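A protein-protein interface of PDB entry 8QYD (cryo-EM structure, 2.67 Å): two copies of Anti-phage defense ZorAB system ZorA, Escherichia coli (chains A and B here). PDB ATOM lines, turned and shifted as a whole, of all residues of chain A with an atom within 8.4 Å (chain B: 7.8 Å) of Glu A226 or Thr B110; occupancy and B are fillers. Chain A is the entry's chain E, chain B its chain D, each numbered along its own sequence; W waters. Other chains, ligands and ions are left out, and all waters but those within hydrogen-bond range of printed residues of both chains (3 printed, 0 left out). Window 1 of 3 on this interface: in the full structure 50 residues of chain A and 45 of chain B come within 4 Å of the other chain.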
ATOM      1  N   ARG A 108      15.386  15.873  31.154  1.00  0.00           N
ATOM      2  CA  ARG A 108      15.232  17.304  31.334  1.00  0.00           C
ATOM      3  C   ARG A 108      13.772  17.641  31.601  1.00  0.00           C
ATOM      4  O   ARG A 108      12.863  16.955  31.128  1.00  0.00           O
ATOM      5  CB  ARG A 108      15.725  18.066  30.102  1.00  0.00           C
ATOM      6  CG  ARG A 108      17.160  17.758  29.718  1.00  0.00           C
ATOM      7  CD  ARG A 108      18.127  18.293  30.752  1.00  0.00           C
ATOM      8  NE  ARG A 108      18.033  19.741  30.878  1.00  0.00           N
ATOM      9  CZ  ARG A 108      18.778  20.604  30.203  1.00  0.00           C
ATOM     10  NH1 ARG A 108      19.709  20.199  29.357  1.00  0.00           N
ATOM     11  NH2 ARG A 108      18.583  21.905  30.380  1.00  0.00           N
ATOM     12  N   ALA A 109      13.557  18.702  32.366  1.00  0.00           N
ATOM     13  CA  ALA A 109      12.222  19.165  32.705  1.00  0.00           C
ATOM     14  C   ALA A 109      11.812  20.295  31.772  1.00  0.00           C
ATOM     15  O   ALA A 109      12.614  21.178  31.459  1.00  0.00           O
ATOM     16  CB  ALA A 109      12.160  19.637  34.157  1.00  0.00           C
ATOM     17  N   SER A 222      15.714  22.102  33.977  1.00  0.00           N
ATOM     18  CA  SER A 222      14.937  22.768  32.948  1.00  0.00           C
ATOM     19  C   SER A 222      15.853  23.571  32.028  1.00  0.00           C
ATOM     20  O   SER A 222      17.077  23.578  32.170  1.00  0.00           O
ATOM     21  CB  SER A 222      13.871  23.660  33.583  1.00  0.00           C
ATOM     22  OG  SER A 222      14.458  24.670  34.382  1.00  0.00           O
ATOM     23  N   GLY A 223      15.248  24.257  31.063  1.00  0.00           N
ATOM     24  CA  GLY A 223      16.005  25.067  30.135  1.00  0.00           C
ATOM     25  C   GLY A 223      16.614  24.322  28.975  1.00  0.00           C
ATOM     26  O   GLY A 223      17.716  24.671  28.541  1.00  0.00           O
ATOM     27  N   VAL A 224      15.933  23.303  28.450  1.00  0.00           N
ATOM     28  CA  VAL A 224      16.519  22.512  27.375  1.00  0.00           C
ATOM     29  C   VAL A 224      16.255  23.141  26.010  1.00  0.00           C
ATOM     30  O   VAL A 224      17.061  22.981  25.086  1.00  0.00           O
ATOM     31  CB  VAL A 224      16.010  21.061  27.450  1.00  0.00           C
ATOM     32  CG1 VAL A 224      14.556  20.969  27.030  1.00  0.00           C
ATOM     33  CG2 VAL A 224      16.876  20.154  26.603  1.00  0.00           C
ATOM     34  N   GLY A 225      15.149  23.870  25.853  1.00  0.00           N
ATOM     35  CA  GLY A 225      14.853  24.478  24.568  1.00  0.00           C
ATOM     36  C   GLY A 225      15.839  25.564  24.184  1.00  0.00           C
ATOM     37  O   GLY A 225      16.247  25.664  23.024  1.00  0.00           O
ATOM     38  N   GLU A 226      16.227  26.401  25.148  1.00  0.00           N
ATOM     39  CA  GLU A 226      17.227  27.424  24.872  1.00  0.00           C
ATOM     40  C   GLU A 226      18.566  26.796  24.517  1.00  0.00           C
ATOM     41  O   GLU A 226      19.282  27.291  23.640  1.00  0.00           O
ATOM     42  CB  GLU A 226      17.373  28.355  26.075  1.00  0.00           C
ATOM     43  CG  GLU A 226      16.314  29.441  26.161  1.00  0.00           C
ATOM     44  CD  GLU A 226      15.030  28.960  26.808  1.00  0.00           C
ATOM     45  OE1 GLU A 226      15.019  27.836  27.352  1.00  0.00           O
ATOM     46  OE2 GLU A 226      14.032  29.709  26.779  1.00  0.00           O
ATOM     47  N   GLU A 227      18.922  25.703  25.192  1.00  0.00           N
ATOM     48  CA  GLU A 227      20.150  24.993  24.857  1.00  0.00           C
ATOM     49  C   GLU A 227      20.090  24.432  23.444  1.00  0.00           C
ATOM     50  O   GLU A 227      21.079  24.481  22.706  1.00  0.00           O
ATOM     51  CB  GLU A 227      20.400  23.877  25.865  1.00  0.00           C
ATOM     52  CG  GLU A 227      20.706  24.365  27.259  1.00  0.00           C
ATOM     53  CD  GLU A 227      20.874  23.229  28.240  1.00  0.00           C
ATOM     54  OE1 GLU A 227      20.926  22.065  27.792  1.00  0.00           O
ATOM     55  OE2 GLU A 227      20.957  23.496  29.457  1.00  0.00           O
ATOM     56  N   TYR A 228      18.934  23.896  23.050  1.00  0.00           N
ATOM     57  CA  TYR A 228      18.778  23.383  21.693  1.00  0.00           C
ATOM     58  C   TYR A 228      18.890  24.496  20.660  1.00  0.00           C
ATOM     59  O   TYR A 228      19.506  24.311  19.606  1.00  0.00           O
ATOM     60  CB  TYR A 228      17.445  22.654  21.563  1.00  0.00           C
ATOM     61  CG  TYR A 228      17.477  21.251  22.115  1.00  0.00           C
ATOM     62  CD1 TYR A 228      18.646  20.512  22.106  1.00  0.00           C
ATOM     63  CD2 TYR A 228      16.339  20.667  22.647  1.00  0.00           C
ATOM     64  CE1 TYR A 228      18.683  19.236  22.607  1.00  0.00           C
ATOM     65  CE2 TYR A 228      16.367  19.389  23.149  1.00  0.00           C
ATOM     66  CZ  TYR A 228      17.543  18.679  23.127  1.00  0.00           C
ATOM     67  OH  TYR A 228      17.583  17.401  23.628  1.00  0.00           O
ATOM     68  N   LEU A 229      18.301  25.660  20.942  1.00  0.00           N
ATOM     69  CA  LEU A 229      18.421  26.788  20.022  1.00  0.00           C
ATOM     70  C   LEU A 229      19.864  27.263  19.907  1.00  0.00           C
ATOM     71  O   LEU A 229      20.334  27.594  18.811  1.00  0.00           O
ATOM     72  CB  LEU A 229      17.521  27.936  20.468  1.00  0.00           C
ATOM     73  CG  LEU A 229      16.017  27.803  20.236  1.00  0.00           C
ATOM     74  CD1 LEU A 229      15.330  29.112  20.561  1.00  0.00           C
ATOM     75  CD2 LEU A 229      15.718  27.379  18.815  1.00  0.00           C
ATOM     76  N   ALA A 230      20.583  27.312  21.030  1.00  0.00           N
ATOM     77  CA  ALA A 230      21.989  27.697  20.989  1.00  0.00           C
ATOM     78  C   ALA A 230      22.804  26.696  20.184  1.00  0.00           C
ATOM     79  O   ALA A 230      23.691  27.081  19.406  1.00  0.00           O
ATOM     80  CB  ALA A 230      22.538  27.821  22.408  1.00  0.00           C
ATOM     81  N   SER A 231      22.516  25.406  20.358  1.00  0.00           N
ATOM     82  CA  SER A 231      23.198  24.375  19.590  1.00  0.00           C
ATOM     83  C   SER A 231      22.917  24.525  18.101  1.00  0.00           C
ATOM     84  O   SER A 231      23.816  24.352  17.274  1.00  0.00           O
ATOM     85  CB  SER A 231      22.770  22.996  20.087  1.00  0.00           C
ATOM     86  OG  SER A 231      23.490  21.970  19.431  1.00  0.00           O
ATOM     87  N   LEU A 232      21.674  24.847  17.742  1.00  0.00           N
ATOM     88  CA  LEU A 232      21.339  25.062  16.337  1.00  0.00           C
ATOM     89  C   LEU A 232      22.089  26.255  15.759  1.00  0.00           C
ATOM     90  O   LEU A 232      22.580  26.198  14.626  1.00  0.00           O
ATOM     91  CB  LEU A 232      19.832  25.258  16.182  1.00  0.00           C
ATOM     92  CG  LEU A 232      18.979  23.994  16.210  1.00  0.00           C
ATOM     93  CD1 LEU A 232      17.511  24.358  16.245  1.00  0.00           C
ATOM     94  CD2 LEU A 232      19.281  23.135  15.008  1.00  0.00           C
ATOM     95  N   VAL A 233      22.174  27.350  16.515  1.00  0.00           N
ATOM     96  CA  VAL A 233      22.899  28.528  16.037  1.00  0.00           C
ATOM     97  C   VAL A 233      24.375  28.201  15.835  1.00  0.00           C
ATOM     98  O   VAL A 233      24.983  28.567  14.812  1.00  0.00           O
ATOM     99  CB  VAL A 233      22.704  29.701  17.014  1.00  0.00           C
ATOM    100  CG1 VAL A 233      23.595  30.861  16.641  1.00  0.00           C
ATOM    101  CG2 VAL A 233      21.255  30.129  17.037  1.00  0.00           C
ATOM    102  N   GLU B  86      16.065  26.313  41.257  1.00  0.00           N
ATOM    103  CA  GLU B  86      15.169  26.347  40.106  1.00  0.00           C
ATOM    104  C   GLU B  86      15.365  27.614  39.284  1.00  0.00           C
ATOM    105  O   GLU B  86      15.348  27.571  38.047  1.00  0.00           O
ATOM    106  CB  GLU B  86      13.720  26.223  40.567  1.00  0.00           C
ATOM    107  CG  GLU B  86      13.431  24.942  41.304  1.00  0.00           C
ATOM    108  CD  GLU B  86      13.891  23.715  40.546  1.00  0.00           C
ATOM    109  OE1 GLU B  86      13.605  23.616  39.336  1.00  0.00           O
ATOM    110  OE2 GLU B  86      14.540  22.845  41.161  1.00  0.00           O
ATOM    111  N   PHE B  87      15.553  28.754  39.952  1.00  0.00           N
ATOM    112  CA  PHE B  87      15.777  29.999  39.224  1.00  0.00           C
ATOM    113  C   PHE B  87      17.046  29.928  38.386  1.00  0.00           C
ATOM    114  O   PHE B  87      17.064  30.372  37.233  1.00  0.00           O
ATOM    115  CB  PHE B  87      15.837  31.169  40.204  1.00  0.00           C
ATOM    116  CG  PHE B  87      16.048  32.498  39.545  1.00  0.00           C
ATOM    117  CD1 PHE B  87      15.106  33.008  38.674  1.00  0.00           C
ATOM    118  CD2 PHE B  87      17.183  33.240  39.805  1.00  0.00           C
ATOM    119  CE1 PHE B  87      15.298  34.228  38.070  1.00  0.00           C
ATOM    120  CE2 PHE B  87      17.380  34.460  39.204  1.00  0.00           C
ATOM    121  CZ  PHE B  87      16.434  34.956  38.336  1.00  0.00           C
ATOM    122  N   GLU B  88      18.120  29.371  38.948  1.00  0.00           N
ATOM    123  CA  GLU B  88      19.363  29.222  38.205  1.00  0.00           C
ATOM    124  C   GLU B  88      19.220  28.219  37.070  1.00  0.00           C
ATOM    125  O   GLU B  88      19.896  28.346  36.044  1.00  0.00           O
ATOM    126  CB  GLU B  88      20.486  28.802  39.149  1.00  0.00           C
ATOM    127  CG  GLU B  88      21.868  28.862  38.536  1.00  0.00           C
ATOM    128  CD  GLU B  88      22.888  28.091  39.342  1.00  0.00           C
ATOM    129  OE1 GLU B  88      22.481  27.228  40.146  1.00  0.00           O
ATOM    130  OE2 GLU B  88      24.098  28.343  39.172  1.00  0.00           O
ATOM    131  N   GLU B  89      18.362  27.210  37.238  1.00  0.00           N
ATOM    132  CA  GLU B  89      18.033  26.338  36.114  1.00  0.00           C
ATOM    133  C   GLU B  89      17.351  27.120  35.000  1.00  0.00           C
ATOM    134  O   GLU B  89      17.598  26.874  33.815  1.00  0.00           O
ATOM    135  CB  GLU B  89      17.144  25.188  36.575  1.00  0.00           C
ATOM    136  CG  GLU B  89      17.874  24.077  37.287  1.00  0.00           C
ATOM    137  CD  GLU B  89      16.932  23.004  37.786  1.00  0.00           C
ATOM    138  OE1 GLU B  89      15.791  22.938  37.288  1.00  0.00           O
ATOM    139  OE2 GLU B  89      17.326  22.226  38.677  1.00  0.00           O
ATOM    140  N   SER B  90      16.480  28.062  35.362  1.00  0.00           N
ATOM    141  CA  SER B  90      15.836  28.902  34.360  1.00  0.00           C
ATOM    142  C   SER B  90      16.799  29.877  33.693  1.00  0.00           C
ATOM    143  O   SER B  90      16.426  30.496  32.692  1.00  0.00           O
ATOM    144  CB  SER B  90      14.679  29.677  34.984  1.00  0.00           C
ATOM    145  OG  SER B  90      15.155  30.660  35.880  1.00  0.00           O
ATOM    146  N   LEU B  91      18.009  30.035  34.220  1.00  0.00           N
ATOM    147  CA  LEU B  91      18.990  30.927  33.619  1.00  0.00           C
ATOM    148  C   LEU B  91      19.722  30.229  32.484  1.00  0.00           C
ATOM    149  O   LEU B  91      20.156  29.081  32.617  1.00  0.00           O
ATOM    150  CB  LEU B  91      19.993  31.402  34.667  1.00  0.00           C
ATOM    151  CG  LEU B  91      19.441  32.272  35.794  1.00  0.00           C
ATOM    152  CD1 LEU B  91      20.550  32.666  36.742  1.00  0.00           C
ATOM    153  CD2 LEU B  91      18.750  33.495  35.231  1.00  0.00           C
ATOM    154  N   HIS B  92      19.867  30.930  31.364  1.00  0.00           N
ATOM    155  CA  HIS B  92      20.542  30.405  30.184  1.00  0.00           C
ATOM    156  C   HIS B  92      21.914  31.057  30.079  1.00  0.00           C
ATOM    157  O   HIS B  92      22.018  32.262  29.832  1.00  0.00           O
ATOM    158  CB  HIS B  92      19.721  30.662  28.924  1.00  0.00           C
ATOM    159  CG  HIS B  92      20.411  30.246  27.664  1.00  0.00           C
ATOM    160  ND1 HIS B  92      20.594  28.925  27.320  1.00  0.00           N
ATOM    161  CD2 HIS B  92      20.967  30.975  26.668  1.00  0.00           C
ATOM    162  CE1 HIS B  92      21.233  28.858  26.166  1.00  0.00           C
ATOM    163  NE2 HIS B  92      21.472  30.088  25.751  1.00  0.00           N
ATOM    164  N   SER B  93      22.963  30.260  30.258  1.00  0.00           N
ATOM    165  CA  SER B  93      24.332  30.743  30.141  1.00  0.00           C
ATOM    166  C   SER B  93      24.770  30.655  28.685  1.00  0.00           C
ATOM    167  O   SER B  93      24.704  29.583  28.076  1.00  0.00           O
ATOM    168  CB  SER B  93      25.271  29.934  31.032  1.00  0.00           C
ATOM    169  OG  SER B  93      24.913  30.052  32.395  1.00  0.00           O
ATOM    170  N   ILE B 107      24.594  35.738  30.754  1.00  0.00           N
ATOM    171  CA  ILE B 107      23.538  34.923  31.337  1.00  0.00           C
ATOM    172  C   ILE B 107      22.211  35.588  31.017  1.00  0.00           C
ATOM    173  O   ILE B 107      22.052  36.796  31.221  1.00  0.00           O
ATOM    174  CB  ILE B 107      23.714  34.746  32.854  1.00  0.00           C
ATOM    175  CG1 ILE B 107      25.058  34.091  33.156  1.00  0.00           C
ATOM    176  CG2 ILE B 107      22.588  33.908  33.420  1.00  0.00           C
ATOM    177  CD1 ILE B 107      25.344  33.971  34.616  1.00  0.00           C
ATOM    178  N   ARG B 108      21.271  34.807  30.502  1.00  0.00           N
ATOM    179  CA  ARG B 108      19.991  35.325  30.052  1.00  0.00           C
ATOM    180  C   ARG B 108      18.868  34.751  30.898  1.00  0.00           C
ATOM    181  O   ARG B 108      18.861  33.560  31.217  1.00  0.00           O
ATOM    182  CB  ARG B 108      19.761  35.005  28.573  1.00  0.00           C
ATOM    183  CG  ARG B 108      20.987  35.224  27.710  1.00  0.00           C
ATOM    184  CD  ARG B 108      21.274  36.703  27.526  1.00  0.00           C
ATOM    185  NE  ARG B 108      20.095  37.438  27.088  1.00  0.00           N
ATOM    186  CZ  ARG B 108      19.934  37.934  25.870  1.00  0.00           C
ATOM    187  NH1 ARG B 108      20.866  37.802  24.942  1.00  0.00           N
ATOM    188  NH2 ARG B 108      18.809  38.575  25.574  1.00  0.00           N
ATOM    189  N   ALA B 109      17.928  35.609  31.272  1.00  0.00           N
ATOM    190  CA  ALA B 109      16.758  35.174  32.015  1.00  0.00           C
ATOM    191  C   ALA B 109      15.712  34.632  31.054  1.00  0.00           C
ATOM    192  O   ALA B 109      15.419  35.252  30.029  1.00  0.00           O
ATOM    193  CB  ALA B 109      16.182  36.328  32.831  1.00  0.00           C
ATOM    194  N   THR B 110      15.159  33.468  31.376  1.00  0.00           N
ATOM    195  CA  THR B 110      14.089  32.883  30.588  1.00  0.00           C
ATOM    196  C   THR B 110      12.762  32.865  31.328  1.00  0.00           C
ATOM    197  O   THR B 110      11.751  32.458  30.750  1.00  0.00           O
ATOM    198  CB  THR B 110      14.465  31.463  30.153  1.00  0.00           C
ATOM    199  OG1 THR B 110      14.593  30.624  31.306  1.00  0.00           O
ATOM    200  CG2 THR B 110      15.782  31.473  29.396  1.00  0.00           C
ATOM    201  N   ALA B 111      12.737  33.299  32.585  1.00  0.00           N
ATOM    202  CA  ALA B 111      11.524  33.338  33.386  1.00  0.00           C
ATOM    203  C   ALA B 111      11.714  34.372  34.480  1.00  0.00           C
ATOM    204  O   ALA B 111      12.847  34.594  34.920  1.00  0.00           O
ATOM    205  CB  ALA B 111      11.216  31.964  33.996  1.00  0.00           C
ATOM    206  N   PRO B 112      10.646  35.027  34.927  1.00  0.00           N
ATOM    207  CA  PRO B 112      10.785  35.983  36.030  1.00  0.00           C
ATOM    208  C   PRO B 112      11.114  35.277  37.332  1.00  0.00           C
ATOM    209  O   PRO B 112      10.743  34.123  37.553  1.00  0.00           O
ATOM    210  CB  PRO B 112       9.409  36.655  36.092  1.00  0.00           C
ATOM    211  CG  PRO B 112       8.482  35.660  35.505  1.00  0.00           C
ATOM    212  CD  PRO B 112       9.257  34.925  34.453  1.00  0.00           C
ATOM    213  N   SER B 113      11.826  35.991  38.206  1.00  0.00           N
ATOM    214  CA  SER B 113      12.204  35.415  39.490  1.00  0.00           C
ATOM    215  C   SER B 113      11.029  35.313  40.449  1.00  0.00           C
ATOM    216  O   SER B 113      11.118  34.577  41.435  1.00  0.00           O
ATOM    217  CB  SER B 113      13.328  36.230  40.128  1.00  0.00           C
ATOM    218  OG  SER B 113      12.920  37.562  40.377  1.00  0.00           O
ATOM    219  N   SER B 115       8.332  33.826  39.821  1.00  0.00           N
ATOM    220  CA  SER B 115       7.766  32.498  39.637  1.00  0.00           C
ATOM    221  C   SER B 115       8.436  31.440  40.500  1.00  0.00           C
ATOM    222  O   SER B 115       7.867  30.360  40.680  1.00  0.00           O
ATOM    223  CB  SER B 115       7.856  32.095  38.166  1.00  0.00           C
ATOM    224  OG  SER B 115       9.164  32.294  37.668  1.00  0.00           O
ATOM    225  N   PHE B 116       9.623  31.717  41.028  1.00  0.00           N
ATOM    226  CA  PHE B 116      10.326  30.806  41.922  1.00  0.00           C
ATOM    227  C   PHE B 116      10.364  31.298  43.356  1.00  0.00           C
ATOM    228  O   PHE B 116      10.223  30.501  44.284  1.00  0.00           O
ATOM    229  CB  PHE B 116      11.756  30.579  41.422  1.00  0.00           C
ATOM    230  CG  PHE B 116      11.837  30.255  39.960  1.00  0.00           C
ATOM    231  CD1 PHE B 116      11.667  28.960  39.514  1.00  0.00           C
ATOM    232  CD2 PHE B 116      12.076  31.250  39.030  1.00  0.00           C
ATOM    233  CE1 PHE B 116      11.738  28.665  38.174  1.00  0.00           C
ATOM    234  CE2 PHE B 116      12.145  30.957  37.689  1.00  0.00           C
ATOM    235  CZ  PHE B 116      11.973  29.663  37.263  1.00  0.00           C
ATOM    236  N   TYR B 220      19.762  39.891  34.938  1.00  0.00           N
ATOM    237  CA  TYR B 220      19.849  39.136  33.699  1.00  0.00           C
ATOM    238  C   TYR B 220      18.766  39.564  32.723  1.00  0.00           C
ATOM    239  O   TYR B 220      17.664  39.949  33.126  1.00  0.00           O
ATOM    240  CB  TYR B 220      19.749  37.639  33.981  1.00  0.00           C
ATOM    241  CG  TYR B 220      20.782  37.172  34.975  1.00  0.00           C
ATOM    242  CD1 TYR B 220      22.132  37.384  34.743  1.00  0.00           C
ATOM    243  CD2 TYR B 220      20.411  36.541  36.151  1.00  0.00           C
ATOM    244  CE1 TYR B 220      23.083  36.972  35.645  1.00  0.00           C
ATOM    245  CE2 TYR B 220      21.359  36.124  37.063  1.00  0.00           C
ATOM    246  CZ  TYR B 220      22.692  36.341  36.802  1.00  0.00           C
ATOM    247  OH  TYR B 220      23.646  35.930  37.700  1.00  0.00           O
ATOM    248  N   ASP B 221      19.089  39.488  31.436  1.00  0.00           N
ATOM    249  CA  ASP B 221      18.214  39.939  30.367  1.00  0.00           C
ATOM    250  C   ASP B 221      17.473  38.764  29.746  1.00  0.00           C
ATOM    251  O   ASP B 221      17.911  37.617  29.825  1.00  0.00           O
ATOM    252  CB  ASP B 221      19.013  40.674  29.293  1.00  0.00           C
ATOM    253  CG  ASP B 221      19.857  41.791  29.863  1.00  0.00           C
ATOM    254  OD1 ASP B 221      19.584  42.225  30.999  1.00  0.00           O
ATOM    255  OD2 ASP B 221      20.799  42.236  29.176  1.00  0.00           O
ATOM    256  N   SER B 222      16.339  39.062  29.129  1.00  0.00           N
ATOM    257  CA  SER B 222      15.492  38.053  28.515  1.00  0.00           C
ATOM    258  C   SER B 222      15.478  38.225  27.000  1.00  0.00           C
ATOM    259  O   SER B 222      16.142  39.099  26.438  1.00  0.00           O
ATOM    260  CB  SER B 222      14.079  38.116  29.096  1.00  0.00           C
ATOM    261  OG  SER B 222      13.457  39.351  28.807  1.00  0.00           O
ATOM    262  N   GLY B 223      14.715  37.362  26.335  1.00  0.00           N
ATOM    263  CA  GLY B 223      14.580  37.419  24.895  1.00  0.00           C
ATOM    264  C   GLY B 223      15.644  36.693  24.109  1.00  0.00           C
ATOM    265  O   GLY B 223      15.889  37.052  22.953  1.00  0.00           O
ATOM    266  N   VAL B 224      16.288  35.681  24.693  1.00  0.00           N
ATOM    267  CA  VAL B 224      17.380  35.012  23.996  1.00  0.00           C
ATOM    268  C   VAL B 224      16.846  34.065  22.926  1.00  0.00           C
ATOM    269  O   VAL B 224      17.526  33.803  21.927  1.00  0.00           O
ATOM    270  CB  VAL B 224      18.285  34.284  25.007  1.00  0.00           C
ATOM    271  CG1 VAL B 224      17.540  33.142  25.681  1.00  0.00           C
ATOM    272  CG2 VAL B 224      19.551  33.804  24.340  1.00  0.00           C
ATOM    273  N   GLY B 225      15.630  33.547  23.103  1.00  0.00           N
ATOM    274  CA  GLY B 225      15.067  32.659  22.101  1.00  0.00           C
ATOM    275  C   GLY B 225      14.786  33.360  20.787  1.00  0.00           C
ATOM    276  O   GLY B 225      15.039  32.810  19.712  1.00  0.00           O
ATOM    277  N   GLU B 226      14.257  34.583  20.851  1.00  0.00           N
ATOM    278  CA  GLU B 226      14.037  35.354  19.634  1.00  0.00           C
ATOM    279  C   GLU B 226      15.355  35.702  18.956  1.00  0.00           C
ATOM    280  O   GLU B 226      15.440  35.708  17.725  1.00  0.00           O
ATOM    281  CB  GLU B 226      13.239  36.618  19.944  1.00  0.00           C
ATOM    282  CG  GLU B 226      11.736  36.416  19.931  1.00  0.00           C
ATOM    283  CD  GLU B 226      11.211  35.826  21.225  1.00  0.00           C
ATOM    284  OE1 GLU B 226      11.975  35.764  22.210  1.00  0.00           O
ATOM    285  OE2 GLU B 226      10.028  35.426  21.257  1.00  0.00           O
ATOM    286  N   TYR B 228      18.051  33.825  19.060  1.00  0.00           N
ATOM    287  CA  TYR B 228      18.489  32.588  18.424  1.00  0.00           C
ATOM    288  C   TYR B 228      17.725  32.331  17.131  1.00  0.00           C
ATOM    289  O   TYR B 228      18.312  31.906  16.129  1.00  0.00           O
ATOM    290  CB  TYR B 228      18.319  31.418  19.389  1.00  0.00           C
ATOM    291  CG  TYR B 228      19.359  31.374  20.481  1.00  0.00           C
ATOM    292  CD1 TYR B 228      20.635  31.867  20.272  1.00  0.00           C
ATOM    293  CD2 TYR B 228      19.063  30.834  21.722  1.00  0.00           C
ATOM    294  CE1 TYR B 228      21.583  31.827  21.265  1.00  0.00           C
ATOM    295  CE2 TYR B 228      20.006  30.786  22.717  1.00  0.00           C
ATOM    296  CZ  TYR B 228      21.265  31.286  22.485  1.00  0.00           C
ATOM    297  OH  TYR B 228      22.214  31.245  23.476  1.00  0.00           O
HETATM  298  O   HOH W   1      19.834  24.374  33.340  1.00  0.00           O
HETATM  299  O   HOH W   2      16.723  28.204  30.042  1.00  0.00           O
HETATM  300  O   HOH W   3      13.831  25.803  36.643  1.00  0.00           O
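The side-chain carboxylate (OE1) of Glu B89 lies close to the backbone NH (N) of Ser A222 (3.4 Å).
N of Thr B110 sits close to O of Ser B90, at 3.5 Å. O of His B92 is in hydrogen-bond range of N of Arg B108. A ring nitrogen (NE2) of His B92 is in hydrogen-bond range of the side-chain hydroxyl (OH) of Tyr B228 (2.7 Å). The backbone carbonyl oxygen (O) of Ser A222 is in hydrogen-bond range of the guanidinium group (NH2) of Arg A108 (2.9 Å).
Among the printed residues, pairs that only touch across the chains: Glu A226 with His B92, Glu A226 with Thr B110, Glu A226 with Val B224, Glu A226 with Tyr B228, Leu A229 with Gly B225, Leu A229 with Tyr B228, Ala A230 with Tyr B228 and Val A233 with Tyr B228.
Glu A226 touches Val B224, but with the chains exchanged Val A224 does not touch Glu B226 (12.7 Å). Glu A226 touches Tyr B228, but with the chains exchanged Tyr A228 does not touch Glu B226 (11.1 Å).
Of the 25 printed residues of chain B, 6 touch a printed residue of chain A. Along chain B the printed residues that touch a printed residue of chain A span positions 89 to 228. Hydrophobic or aromatic side chains of chain A that line the printed part of chain B: Leu A229, Ala A230 and Val A233.
Of the printed residues of chain B, Ser A222 touches Glu B89. No residue of chain B comes within 4 Å of Gly A225. Of chain B, only His B92 (3.5 Å), Thr B110 (3.6 Å), Val B224 (3.9 Å) and Tyr B228 (3.7 Å) come within 4 Å of Glu A226. Tyr A228 touches none of the printed residues of chain B. Printed residues of chain B within 4 Å of Leu A229: Gly B225 (3.8 Å) and Tyr B228 (3.5 Å). Glu B88 touches none of the printed residues of chain A. Of the printed residues of chain A, Glu B89 touches Ser A222. Printed residues of chain A within 4 Å of His B92: Glu A226. No residue of chain A comes within 4 Å of Ala B109. Of chain A, only Glu A226 (3.6 Å) comes within 4 Å of Thr B110. No residue of chain A comes within 4 Å of Ala B111. Of the printed residues of chain A, Gly B225 touches Leu A229. The nearest residue of chain B that does not touch Glu A226 is Gly B225 (5.2 Å). The nearest residue of chain A that does not touch Thr B110 is Gly A223 (5.9 Å). The nearest printed residue of chain B that does not touch Ser A222 is Ser B90 (4.1 Å).
Water W3 lies within hydrogen-bond range of OG of Ser A222 and O of Glu B86. Water W1 bridges the backbone carbonyl oxygen of Ser A222 (3.1 Å) and the backbone carbonyl oxygen of Glu B89 (3.4 Å). Water W2 bridges the side-chain carboxylate of Glu A226 and the side-chain hydroxyl of Thr B110.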
